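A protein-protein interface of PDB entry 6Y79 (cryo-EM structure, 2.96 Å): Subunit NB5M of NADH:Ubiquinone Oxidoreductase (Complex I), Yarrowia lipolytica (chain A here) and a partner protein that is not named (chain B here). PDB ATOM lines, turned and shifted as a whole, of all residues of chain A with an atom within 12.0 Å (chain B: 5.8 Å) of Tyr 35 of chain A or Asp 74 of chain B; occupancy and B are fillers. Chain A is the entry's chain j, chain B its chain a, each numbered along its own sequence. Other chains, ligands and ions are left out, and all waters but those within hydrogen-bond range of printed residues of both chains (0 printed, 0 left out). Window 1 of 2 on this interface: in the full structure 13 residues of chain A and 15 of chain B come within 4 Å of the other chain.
OD1 of Asp 29 of chain A lies within hydrogen-bond range of N of Ile 32 of chain A (3.3 Å). The side-chain hydroxyl of Tyr 35 of chain A lies within hydrogen-bond range of the guanidinium group of Arg 39 of chain A, 2.5 Å away. The guanidinium group (NH1) of Arg 45 of chain A lies within hydrogen-bond range of the backbone carbonyl oxygen (O) of Trp 38 of chain A, 2.5 Å away.
Among the printed residues, pairs that only touch across the chains: Tyr 35 of chain A with Ser 71 of chain B, Tyr 35 of chain A with Tyr 40 of chain B, Trp 38 of chain A with Val 72 of chain B, Tyr 35 of chain A with Asp 74 of chain B, Trp 38 of chain A with Tyr 40 of chain B and Ile 32 of chain A with Leu 70 of chain B.
Asp 74 of chain B touches just one residue of chain A: Tyr 35 (3.6 Å). Ser 71 of chain B touches just one residue of chain A: Tyr 35. Of chain A, only Trp 38 (3.6 Å) comes within 4 Å of Val 72 of chain B. No residue of chain A comes within 4 Å of Asp 75 of chain B. No residue of chain A comes within 4 Å of Leu 76 of chain B. Asp 78 of chain B touches none of the printed residues of chain A. Of the printed residues of chain B, Trp 38 of chain A touches Tyr 40 (3.7 Å) and Val 72 (3.6 Å). Of the printed residues of chain B, Ile 32 of chain A touches Leu 70 (3.9 Å). Of the printed residues of chain A, Tyr 40 of chain B touches Tyr 35 and Trp 38. Arg 39 of chain A touches none of the printed residues of chain B.
Hydrophobic or aromatic side chains of chain A that line the printed part of chain B: Ile 32, Tyr 35 and Trp 38. Printed residues of chain B that touch a printed residue of chain A: Tyr 40, Leu 70, Ser 71, Val 72 and Asp 74. Among the printed residues, 6 pairs touch across the chains. Among the printed residues, no Asp or Glu carboxylate lies within 4 Å of a Lys or Arg side-chain nitrogen of the other chain.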
ATOM      1  N   ASN A  28      14.778  24.415 -20.955  1.00  0.00           N
ATOM      2  CA  ASN A  28      15.821  24.622 -19.969  1.00  0.00           C
ATOM      3  C   ASN A  28      15.775  23.516 -18.932  1.00  0.00           C
ATOM      4  O   ASN A  28      14.713  22.979 -18.592  1.00  0.00           O
ATOM      5  CB  ASN A  28      15.660  25.948 -19.253  1.00  0.00           C
ATOM      6  CG  ASN A  28      15.709  27.135 -20.198  1.00  0.00           C
ATOM      7  OD1 ASN A  28      14.689  27.783 -20.443  1.00  0.00           O
ATOM      8  ND2 ASN A  28      16.896  27.461 -20.691  1.00  0.00           N
ATOM      9  N   ASP A  29      16.956  23.135 -18.475  1.00  0.00           N
ATOM     10  CA  ASP A  29      17.112  22.279 -17.303  1.00  0.00           C
ATOM     11  C   ASP A  29      17.707  23.090 -16.177  1.00  0.00           C
ATOM     12  O   ASP A  29      18.798  23.633 -16.319  1.00  0.00           O
ATOM     13  CB  ASP A  29      17.981  21.067 -17.621  1.00  0.00           C
ATOM     14  CG  ASP A  29      18.034  20.010 -16.503  1.00  0.00           C
ATOM     15  OD1 ASP A  29      17.885  20.254 -15.310  1.00  0.00           O
ATOM     16  OD2 ASP A  29      18.027  18.827 -16.930  1.00  0.00           O
ATOM     17  N   GLY A  30      16.974  23.169 -15.068  1.00  0.00           N
ATOM     18  CA  GLY A  30      17.457  23.924 -13.931  1.00  0.00           C
ATOM     19  C   GLY A  30      18.693  23.313 -13.304  1.00  0.00           C
ATOM     20  O   GLY A  30      19.603  24.029 -12.885  1.00  0.00           O
ATOM     21  N   ALA A  31      18.763  21.983 -13.278  1.00  0.00           N
ATOM     22  CA  ALA A  31      19.917  21.314 -12.684  1.00  0.00           C
ATOM     23  C   ALA A  31      21.158  21.458 -13.553  1.00  0.00           C
ATOM     24  O   ALA A  31      22.250  21.712 -13.035  1.00  0.00           O
ATOM     25  CB  ALA A  31      19.609  19.839 -12.438  1.00  0.00           C
ATOM     26  N   ILE A  32      21.014  21.319 -14.874  1.00  0.00           N
ATOM     27  CA  ILE A  32      22.160  21.471 -15.767  1.00  0.00           C
ATOM     28  C   ILE A  32      22.621  22.922 -15.802  1.00  0.00           C
ATOM     29  O   ILE A  32      23.826  23.199 -15.824  1.00  0.00           O
ATOM     30  CB  ILE A  32      21.819  20.936 -17.172  1.00  0.00           C
ATOM     31  CG1 ILE A  32      21.461  19.455 -17.106  1.00  0.00           C
ATOM     32  CG2 ILE A  32      22.984  21.101 -18.132  1.00  0.00           C
ATOM     33  CD1 ILE A  32      21.048  18.883 -18.430  1.00  0.00           C
ATOM     34  N   ASP A  33      21.679  23.871 -15.760  1.00  0.00           N
ATOM     35  CA  ASP A  33      22.048  25.284 -15.742  1.00  0.00           C
ATOM     36  C   ASP A  33      22.753  25.658 -14.449  1.00  0.00           C
ATOM     37  O   ASP A  33      23.735  26.405 -14.473  1.00  0.00           O
ATOM     38  CB  ASP A  33      20.820  26.169 -15.948  1.00  0.00           C
ATOM     39  CG  ASP A  33      20.289  26.115 -17.364  1.00  0.00           C
ATOM     40  OD1 ASP A  33      21.046  25.713 -18.268  1.00  0.00           O
ATOM     41  OD2 ASP A  33      19.108  26.461 -17.573  1.00  0.00           O
ATOM     42  N   ARG A  34      22.294  25.123 -13.315  1.00  0.00           N
ATOM     43  CA  ARG A  34      22.953  25.411 -12.044  1.00  0.00           C
ATOM     44  C   ARG A  34      24.322  24.751 -11.963  1.00  0.00           C
ATOM     45  O   ARG A  34      25.274  25.350 -11.454  1.00  0.00           O
ATOM     46  CB  ARG A  34      22.073  24.960 -10.881  1.00  0.00           C
ATOM     47  CG  ARG A  34      20.924  25.906 -10.582  1.00  0.00           C
ATOM     48  CD  ARG A  34      20.157  25.491  -9.338  1.00  0.00           C
ATOM     49  NE  ARG A  34      19.701  24.105  -9.397  1.00  0.00           N
ATOM     50  CZ  ARG A  34      18.492  23.728  -9.801  1.00  0.00           C
ATOM     51  NH1 ARG A  34      18.171  22.442  -9.818  1.00  0.00           N
ATOM     52  NH2 ARG A  34      17.604  24.634 -10.189  1.00  0.00           N
ATOM     53  N   TYR A  35      24.445  23.535 -12.495  1.00  0.00           N
ATOM     54  CA  TYR A  35      25.726  22.838 -12.547  1.00  0.00           C
ATOM     55  C   TYR A  35      26.732  23.583 -13.413  1.00  0.00           C
ATOM     56  O   TYR A  35      27.895  23.757 -13.034  1.00  0.00           O
ATOM     57  CB  TYR A  35      25.497  21.431 -13.086  1.00  0.00           C
ATOM     58  CG  TYR A  35      26.743  20.648 -13.357  1.00  0.00           C
ATOM     59  CD1 TYR A  35      27.540  20.220 -12.321  1.00  0.00           C
ATOM     60  CD2 TYR A  35      27.106  20.308 -14.651  1.00  0.00           C
ATOM     61  CE1 TYR A  35      28.676  19.498 -12.557  1.00  0.00           C
ATOM     62  CE2 TYR A  35      28.244  19.575 -14.898  1.00  0.00           C
ATOM     63  CZ  TYR A  35      29.022  19.173 -13.845  1.00  0.00           C
ATOM     64  OH  TYR A  35      30.160  18.446 -14.077  1.00  0.00           O
ATOM     65  N   ALA A  36      26.290  24.054 -14.574  1.00  0.00           N
ATOM     66  CA  ALA A  36      27.202  24.710 -15.490  1.00  0.00           C
ATOM     67  C   ALA A  36      27.556  26.111 -15.038  1.00  0.00           C
ATOM     68  O   ALA A  36      28.695  26.546 -15.233  1.00  0.00           O
ATOM     69  CB  ALA A  36      26.593  24.748 -16.875  1.00  0.00           C
ATOM     70  N   HIS A  37      26.606  26.831 -14.438  1.00  0.00           N
ATOM     71  CA  HIS A  37      26.931  28.104 -13.817  1.00  0.00           C
ATOM     72  C   HIS A  37      27.867  27.920 -12.638  1.00  0.00           C
ATOM     73  O   HIS A  37      28.655  28.815 -12.326  1.00  0.00           O
ATOM     74  CB  HIS A  37      25.660  28.811 -13.363  1.00  0.00           C
ATOM     75  CG  HIS A  37      25.889  30.207 -12.882  1.00  0.00           C
ATOM     76  ND1 HIS A  37      26.338  30.488 -11.610  1.00  0.00           N
ATOM     77  CD2 HIS A  37      25.738  31.399 -13.501  1.00  0.00           C
ATOM     78  CE1 HIS A  37      26.450  31.795 -11.467  1.00  0.00           C
ATOM     79  NE2 HIS A  37      26.091  32.371 -12.599  1.00  0.00           N
ATOM     80  N   TRP A  38      27.796  26.772 -11.975  1.00  0.00           N
ATOM     81  CA  TRP A  38      28.725  26.494 -10.898  1.00  0.00           C
ATOM     82  C   TRP A  38      30.124  26.203 -11.418  1.00  0.00           C
ATOM     83  O   TRP A  38      31.108  26.562 -10.761  1.00  0.00           O
ATOM     84  CB  TRP A  38      28.204  25.322 -10.073  1.00  0.00           C
ATOM     85  CG  TRP A  38      29.021  25.069  -8.884  1.00  0.00           C
ATOM     86  CD1 TRP A  38      28.867  25.633  -7.663  1.00  0.00           C
ATOM     87  CD2 TRP A  38      30.144  24.198  -8.787  1.00  0.00           C
ATOM     88  NE1 TRP A  38      29.822  25.167  -6.806  1.00  0.00           N
ATOM     89  CE2 TRP A  38      30.624  24.285  -7.475  1.00  0.00           C
ATOM     90  CE3 TRP A  38      30.794  23.356  -9.685  1.00  0.00           C
ATOM     91  CZ2 TRP A  38      31.717  23.560  -7.037  1.00  0.00           C
ATOM     92  CZ3 TRP A  38      31.878  22.643  -9.249  1.00  0.00           C
ATOM     93  CH2 TRP A  38      32.331  22.748  -7.939  1.00  0.00           C
ATOM     94  N   ARG A  39      30.232  25.528 -12.568  1.00  0.00           N
ATOM     95  CA  ARG A  39      31.546  25.166 -13.099  1.00  0.00           C
ATOM     96  C   ARG A  39      32.230  26.335 -13.797  1.00  0.00           C
ATOM     97  O   ARG A  39      33.458  26.452 -13.741  1.00  0.00           O
ATOM     98  CB  ARG A  39      31.419  24.007 -14.076  1.00  0.00           C
ATOM     99  CG  ARG A  39      30.976  22.689 -13.496  1.00  0.00           C
ATOM    100  CD  ARG A  39      32.099  21.999 -12.773  1.00  0.00           C
ATOM    101  NE  ARG A  39      33.173  21.641 -13.688  1.00  0.00           N
ATOM    102  CZ  ARG A  39      33.264  20.487 -14.335  1.00  0.00           C
ATOM    103  NH1 ARG A  39      34.279  20.266 -15.152  1.00  0.00           N
ATOM    104  NH2 ARG A  39      32.345  19.553 -14.173  1.00  0.00           N
ATOM    105  N   THR A  40      31.454  27.162 -14.509  1.00  0.00           N
ATOM    106  CA  THR A  40      31.997  28.313 -15.226  1.00  0.00           C
ATOM    107  C   THR A  40      32.653  29.308 -14.281  1.00  0.00           C
ATOM    108  O   THR A  40      33.729  29.836 -14.583  1.00  0.00           O
ATOM    109  CB  THR A  40      30.884  28.998 -16.022  1.00  0.00           C
ATOM    110  OG1 THR A  40      30.292  28.061 -16.925  1.00  0.00           O
ATOM    111  CG2 THR A  40      31.410  30.181 -16.825  1.00  0.00           C
ATOM    112  N   PHE A  41      32.051  29.545 -13.124  1.00  0.00           N
ATOM    113  CA  PHE A  41      32.547  30.521 -12.166  1.00  0.00           C
ATOM    114  C   PHE A  41      33.215  29.844 -10.979  1.00  0.00           C
ATOM    115  O   PHE A  41      33.073  30.289  -9.841  1.00  0.00           O
ATOM    116  CB  PHE A  41      31.409  31.431 -11.718  1.00  0.00           C
ATOM    117  CG  PHE A  41      30.830  32.257 -12.834  1.00  0.00           C
ATOM    118  CD1 PHE A  41      31.621  32.668 -13.896  1.00  0.00           C
ATOM    119  CD2 PHE A  41      29.494  32.598 -12.838  1.00  0.00           C
ATOM    120  CE1 PHE A  41      31.093  33.406 -14.924  1.00  0.00           C
ATOM    121  CE2 PHE A  41      28.960  33.344 -13.870  1.00  0.00           C
ATOM    122  CZ  PHE A  41      29.763  33.746 -14.911  1.00  0.00           C
ATOM    123  N   TYR A  42      33.966  28.773 -11.252  1.00  0.00           N
ATOM    124  CA  TYR A  42      34.541  27.925 -10.211  1.00  0.00           C
ATOM    125  C   TYR A  42      35.630  28.639  -9.431  1.00  0.00           C
ATOM    126  O   TYR A  42      35.918  28.279  -8.288  1.00  0.00           O
ATOM    127  CB  TYR A  42      35.101  26.656 -10.851  1.00  0.00           C
ATOM    128  CG  TYR A  42      35.780  25.693  -9.909  1.00  0.00           C
ATOM    129  CD1 TYR A  42      35.041  24.819  -9.140  1.00  0.00           C
ATOM    130  CD2 TYR A  42      37.163  25.658  -9.797  1.00  0.00           C
ATOM    131  CE1 TYR A  42      35.654  23.939  -8.282  1.00  0.00           C
ATOM    132  CE2 TYR A  42      37.785  24.788  -8.940  1.00  0.00           C
ATOM    133  CZ  TYR A  42      37.027  23.929  -8.187  1.00  0.00           C
ATOM    134  OH  TYR A  42      37.643  23.052  -7.334  1.00  0.00           O
ATOM    135  N   GLN A  43      36.235  29.650 -10.029  1.00  0.00           N
ATOM    136  CA  GLN A  43      37.427  30.271  -9.482  1.00  0.00           C
ATOM    137  C   GLN A  43      37.142  31.224  -8.336  1.00  0.00           C
ATOM    138  O   GLN A  43      38.039  31.485  -7.532  1.00  0.00           O
ATOM    139  CB  GLN A  43      38.128  31.022 -10.589  1.00  0.00           C
ATOM    140  CG  GLN A  43      37.292  32.144 -11.186  1.00  0.00           C
ATOM    141  CD  GLN A  43      36.516  31.726 -12.396  1.00  0.00           C
ATOM    142  OE1 GLN A  43      36.460  30.551 -12.731  1.00  0.00           O
ATOM    143  NE2 GLN A  43      35.902  32.690 -13.063  1.00  0.00           N
ATOM    144  N   ARG A  45      35.076  30.695  -5.968  1.00  0.00           N
ATOM    145  CA  ARG A  45      34.878  29.871  -4.789  1.00  0.00           C
ATOM    146  C   ARG A  45      36.037  28.909  -4.591  1.00  0.00           C
ATOM    147  O   ARG A  45      35.964  28.036  -3.724  1.00  0.00           O
ATOM    148  CB  ARG A  45      33.556  29.109  -4.891  1.00  0.00           C
ATOM    149  CG  ARG A  45      33.500  28.148  -6.053  1.00  0.00           C
ATOM    150  CD  ARG A  45      32.160  27.470  -6.138  1.00  0.00           C
ATOM    151  NE  ARG A  45      31.094  28.397  -6.488  1.00  0.00           N
ATOM    152  CZ  ARG A  45      30.736  28.666  -7.736  1.00  0.00           C
ATOM    153  NH1 ARG A  45      31.362  28.069  -8.738  1.00  0.00           N
ATOM    154  NH2 ARG A  45      29.752  29.521  -7.987  1.00  0.00           N
ATOM    155  N   TYR B  40      25.703  24.696  -2.908  1.00  0.00           N
ATOM    156  CA  TYR B  40      25.671  23.579  -3.841  1.00  0.00           C
ATOM    157  C   TYR B  40      25.443  22.279  -3.072  1.00  0.00           C
ATOM    158  O   TYR B  40      26.150  22.032  -2.080  1.00  0.00           O
ATOM    159  CB  TYR B  40      26.959  23.503  -4.664  1.00  0.00           C
ATOM    160  CG  TYR B  40      26.833  22.583  -5.849  1.00  0.00           C
ATOM    161  CD1 TYR B  40      26.264  23.018  -7.041  1.00  0.00           C
ATOM    162  CD2 TYR B  40      27.242  21.268  -5.768  1.00  0.00           C
ATOM    163  CE1 TYR B  40      26.126  22.164  -8.119  1.00  0.00           C
ATOM    164  CE2 TYR B  40      27.073  20.415  -6.820  1.00  0.00           C
ATOM    165  CZ  TYR B  40      26.550  20.869  -8.003  1.00  0.00           C
ATOM    166  OH  TYR B  40      26.423  20.005  -9.059  1.00  0.00           O
ATOM    167  N   LEU B  70      22.876  17.218 -10.241  1.00  0.00           N
ATOM    168  CA  LEU B  70      24.117  16.662 -10.752  1.00  0.00           C
ATOM    169  C   LEU B  70      25.237  16.867  -9.750  1.00  0.00           C
ATOM    170  O   LEU B  70      25.393  17.960  -9.204  1.00  0.00           O
ATOM    171  CB  LEU B  70      24.496  17.312 -12.078  1.00  0.00           C
ATOM    172  CG  LEU B  70      23.471  17.116 -13.181  1.00  0.00           C
ATOM    173  CD1 LEU B  70      23.878  17.875 -14.415  1.00  0.00           C
ATOM    174  CD2 LEU B  70      23.328  15.637 -13.477  1.00  0.00           C
ATOM    175  N   SER B  71      26.034  15.824  -9.552  1.00  0.00           N
ATOM    176  CA  SER B  71      27.210  15.845  -8.703  1.00  0.00           C
ATOM    177  C   SER B  71      28.258  16.802  -9.250  1.00  0.00           C
ATOM    178  O   SER B  71      28.208  17.226 -10.401  1.00  0.00           O
ATOM    179  CB  SER B  71      27.800  14.446  -8.601  1.00  0.00           C
ATOM    180  OG  SER B  71      29.109  14.469  -8.065  1.00  0.00           O
ATOM    181  N   VAL B  72      29.212  17.178  -8.404  1.00  0.00           N
ATOM    182  CA  VAL B  72      30.438  17.734  -8.949  1.00  0.00           C
ATOM    183  C   VAL B  72      31.230  16.563  -9.497  1.00  0.00           C
ATOM    184  O   VAL B  72      31.164  15.453  -8.949  1.00  0.00           O
ATOM    185  CB  VAL B  72      31.204  18.527  -7.877  1.00  0.00           C
ATOM    186  CG1 VAL B  72      32.416  19.197  -8.445  1.00  0.00           C
ATOM    187  CG2 VAL B  72      30.356  19.568  -7.336  1.00  0.00           C
ATOM    188  N   ASN B  73      31.940  16.795 -10.609  1.00  0.00           N
ATOM    189  CA  ASN B  73      32.601  15.753 -11.399  1.00  0.00           C
ATOM    190  C   ASN B  73      31.586  14.724 -11.877  1.00  0.00           C
ATOM    191  O   ASN B  73      31.788  13.516 -11.767  1.00  0.00           O
ATOM    192  CB  ASN B  73      33.761  15.109 -10.637  1.00  0.00           C
ATOM    193  CG  ASN B  73      34.627  16.138  -9.960  1.00  0.00           C
ATOM    194  OD1 ASN B  73      34.745  17.264 -10.433  1.00  0.00           O
ATOM    195  ND2 ASN B  73      35.216  15.774  -8.835  1.00  0.00           N
ATOM    196  N   ASP B  74      30.474  15.237 -12.403  1.00  0.00           N
ATOM    197  CA  ASP B  74      29.393  14.416 -12.916  1.00  0.00           C
ATOM    198  C   ASP B  74      29.760  13.710 -14.210  1.00  0.00           C
ATOM    199  O   ASP B  74      29.226  12.633 -14.486  1.00  0.00           O
ATOM    200  CB  ASP B  74      28.157  15.282 -13.123  1.00  0.00           C
ATOM    201  CG  ASP B  74      26.957  14.485 -13.561  1.00  0.00           C
ATOM    202  OD1 ASP B  74      26.556  13.556 -12.824  1.00  0.00           O
ATOM    203  OD2 ASP B  74      26.424  14.777 -14.651  1.00  0.00           O
ATOM    204  N   ASP B  75      30.684  14.259 -14.994  1.00  0.00           N
ATOM    205  CA  ASP B  75      31.086  13.576 -16.216  1.00  0.00           C
ATOM    206  C   ASP B  75      32.008  12.392 -15.958  1.00  0.00           C
ATOM    207  O   ASP B  75      32.370  11.694 -16.907  1.00  0.00           O
ATOM    208  CB  ASP B  75      31.734  14.556 -17.199  1.00  0.00           C
ATOM    209  CG  ASP B  75      32.929  15.282 -16.623  1.00  0.00           C
ATOM    210  OD1 ASP B  75      33.129  15.251 -15.395  1.00  0.00           O
ATOM    211  OD2 ASP B  75      33.681  15.888 -17.415  1.00  0.00           O
ATOM    212  N   LEU B  76      32.390  12.151 -14.707  1.00  0.00           N
ATOM    213  CA  LEU B  76      32.983  10.891 -14.300  1.00  0.00           C
ATOM    214  C   LEU B  76      31.949   9.877 -13.836  1.00  0.00           C
ATOM    215  O   LEU B  76      32.287   8.702 -13.672  1.00  0.00           O
ATOM    216  CB  LEU B  76      34.006  11.133 -13.196  1.00  0.00           C
ATOM    217  CG  LEU B  76      35.211  11.939 -13.668  1.00  0.00           C
ATOM    218  CD1 LEU B  76      36.209  12.096 -12.558  1.00  0.00           C
ATOM    219  CD2 LEU B  76      35.856  11.269 -14.859  1.00  0.00           C
ATOM    220  N   TYR B  77      30.699  10.295 -13.649  1.00  0.00           N
ATOM    221  CA  TYR B  77      29.622   9.400 -13.254  1.00  0.00           C
ATOM    222  C   TYR B  77      28.484   9.428 -14.259  1.00  0.00           C
ATOM    223  O   TYR B  77      27.355   9.057 -13.930  1.00  0.00           O
ATOM    224  CB  TYR B  77      29.120   9.763 -11.859  1.00  0.00           C
ATOM    225  CG  TYR B  77      30.170   9.540 -10.817  1.00  0.00           C
ATOM    226  CD1 TYR B  77      30.397   8.275 -10.305  1.00  0.00           C
ATOM    227  CD2 TYR B  77      30.959  10.583 -10.369  1.00  0.00           C
ATOM    228  CE1 TYR B  77      31.369   8.057  -9.360  1.00  0.00           C
ATOM    229  CE2 TYR B  77      31.942  10.377  -9.437  1.00  0.00           C
ATOM    230  CZ  TYR B  77      32.134   9.112  -8.926  1.00  0.00           C
ATOM    231  OH  TYR B  77      33.105   8.897  -7.982  1.00  0.00           O
ATOM    232  N   ASP B  78      28.763   9.870 -15.473  1.00  0.00           N
ATOM    233  CA  ASP B  78      27.766   9.895 -16.519  1.00  0.00           C
ATOM    234  C   ASP B  78      27.752   8.551 -17.242  1.00  0.00           C
ATOM    235  O   ASP B  78      28.559   7.657 -16.989  1.00  0.00           O
ATOM    236  CB  ASP B  78      28.051  11.052 -17.481  1.00  0.00           C
ATOM    237  CG  ASP B  78      26.853  11.422 -18.351  1.00  0.00           C
ATOM    238  OD1 ASP B  78      25.759  10.860 -18.126  1.00  0.00           O
ATOM    239  OD2 ASP B  78      27.014  12.256 -19.263  1.00  0.00           O
ATOM    240  N   SER B  81      30.857   8.138 -19.452  1.00  0.00           N
ATOM    241  CA  SER B  81      32.071   7.995 -18.668  1.00  0.00           C
ATOM    242  C   SER B  81      32.631   6.594 -18.949  1.00  0.00           C
ATOM    243  O   SER B  81      32.038   5.828 -19.696  1.00  0.00           O
ATOM    244  CB  SER B  81      31.698   8.238 -17.210  1.00  0.00           C
ATOM    245  OG  SER B  81      32.801   8.247 -16.334  1.00  0.00           O
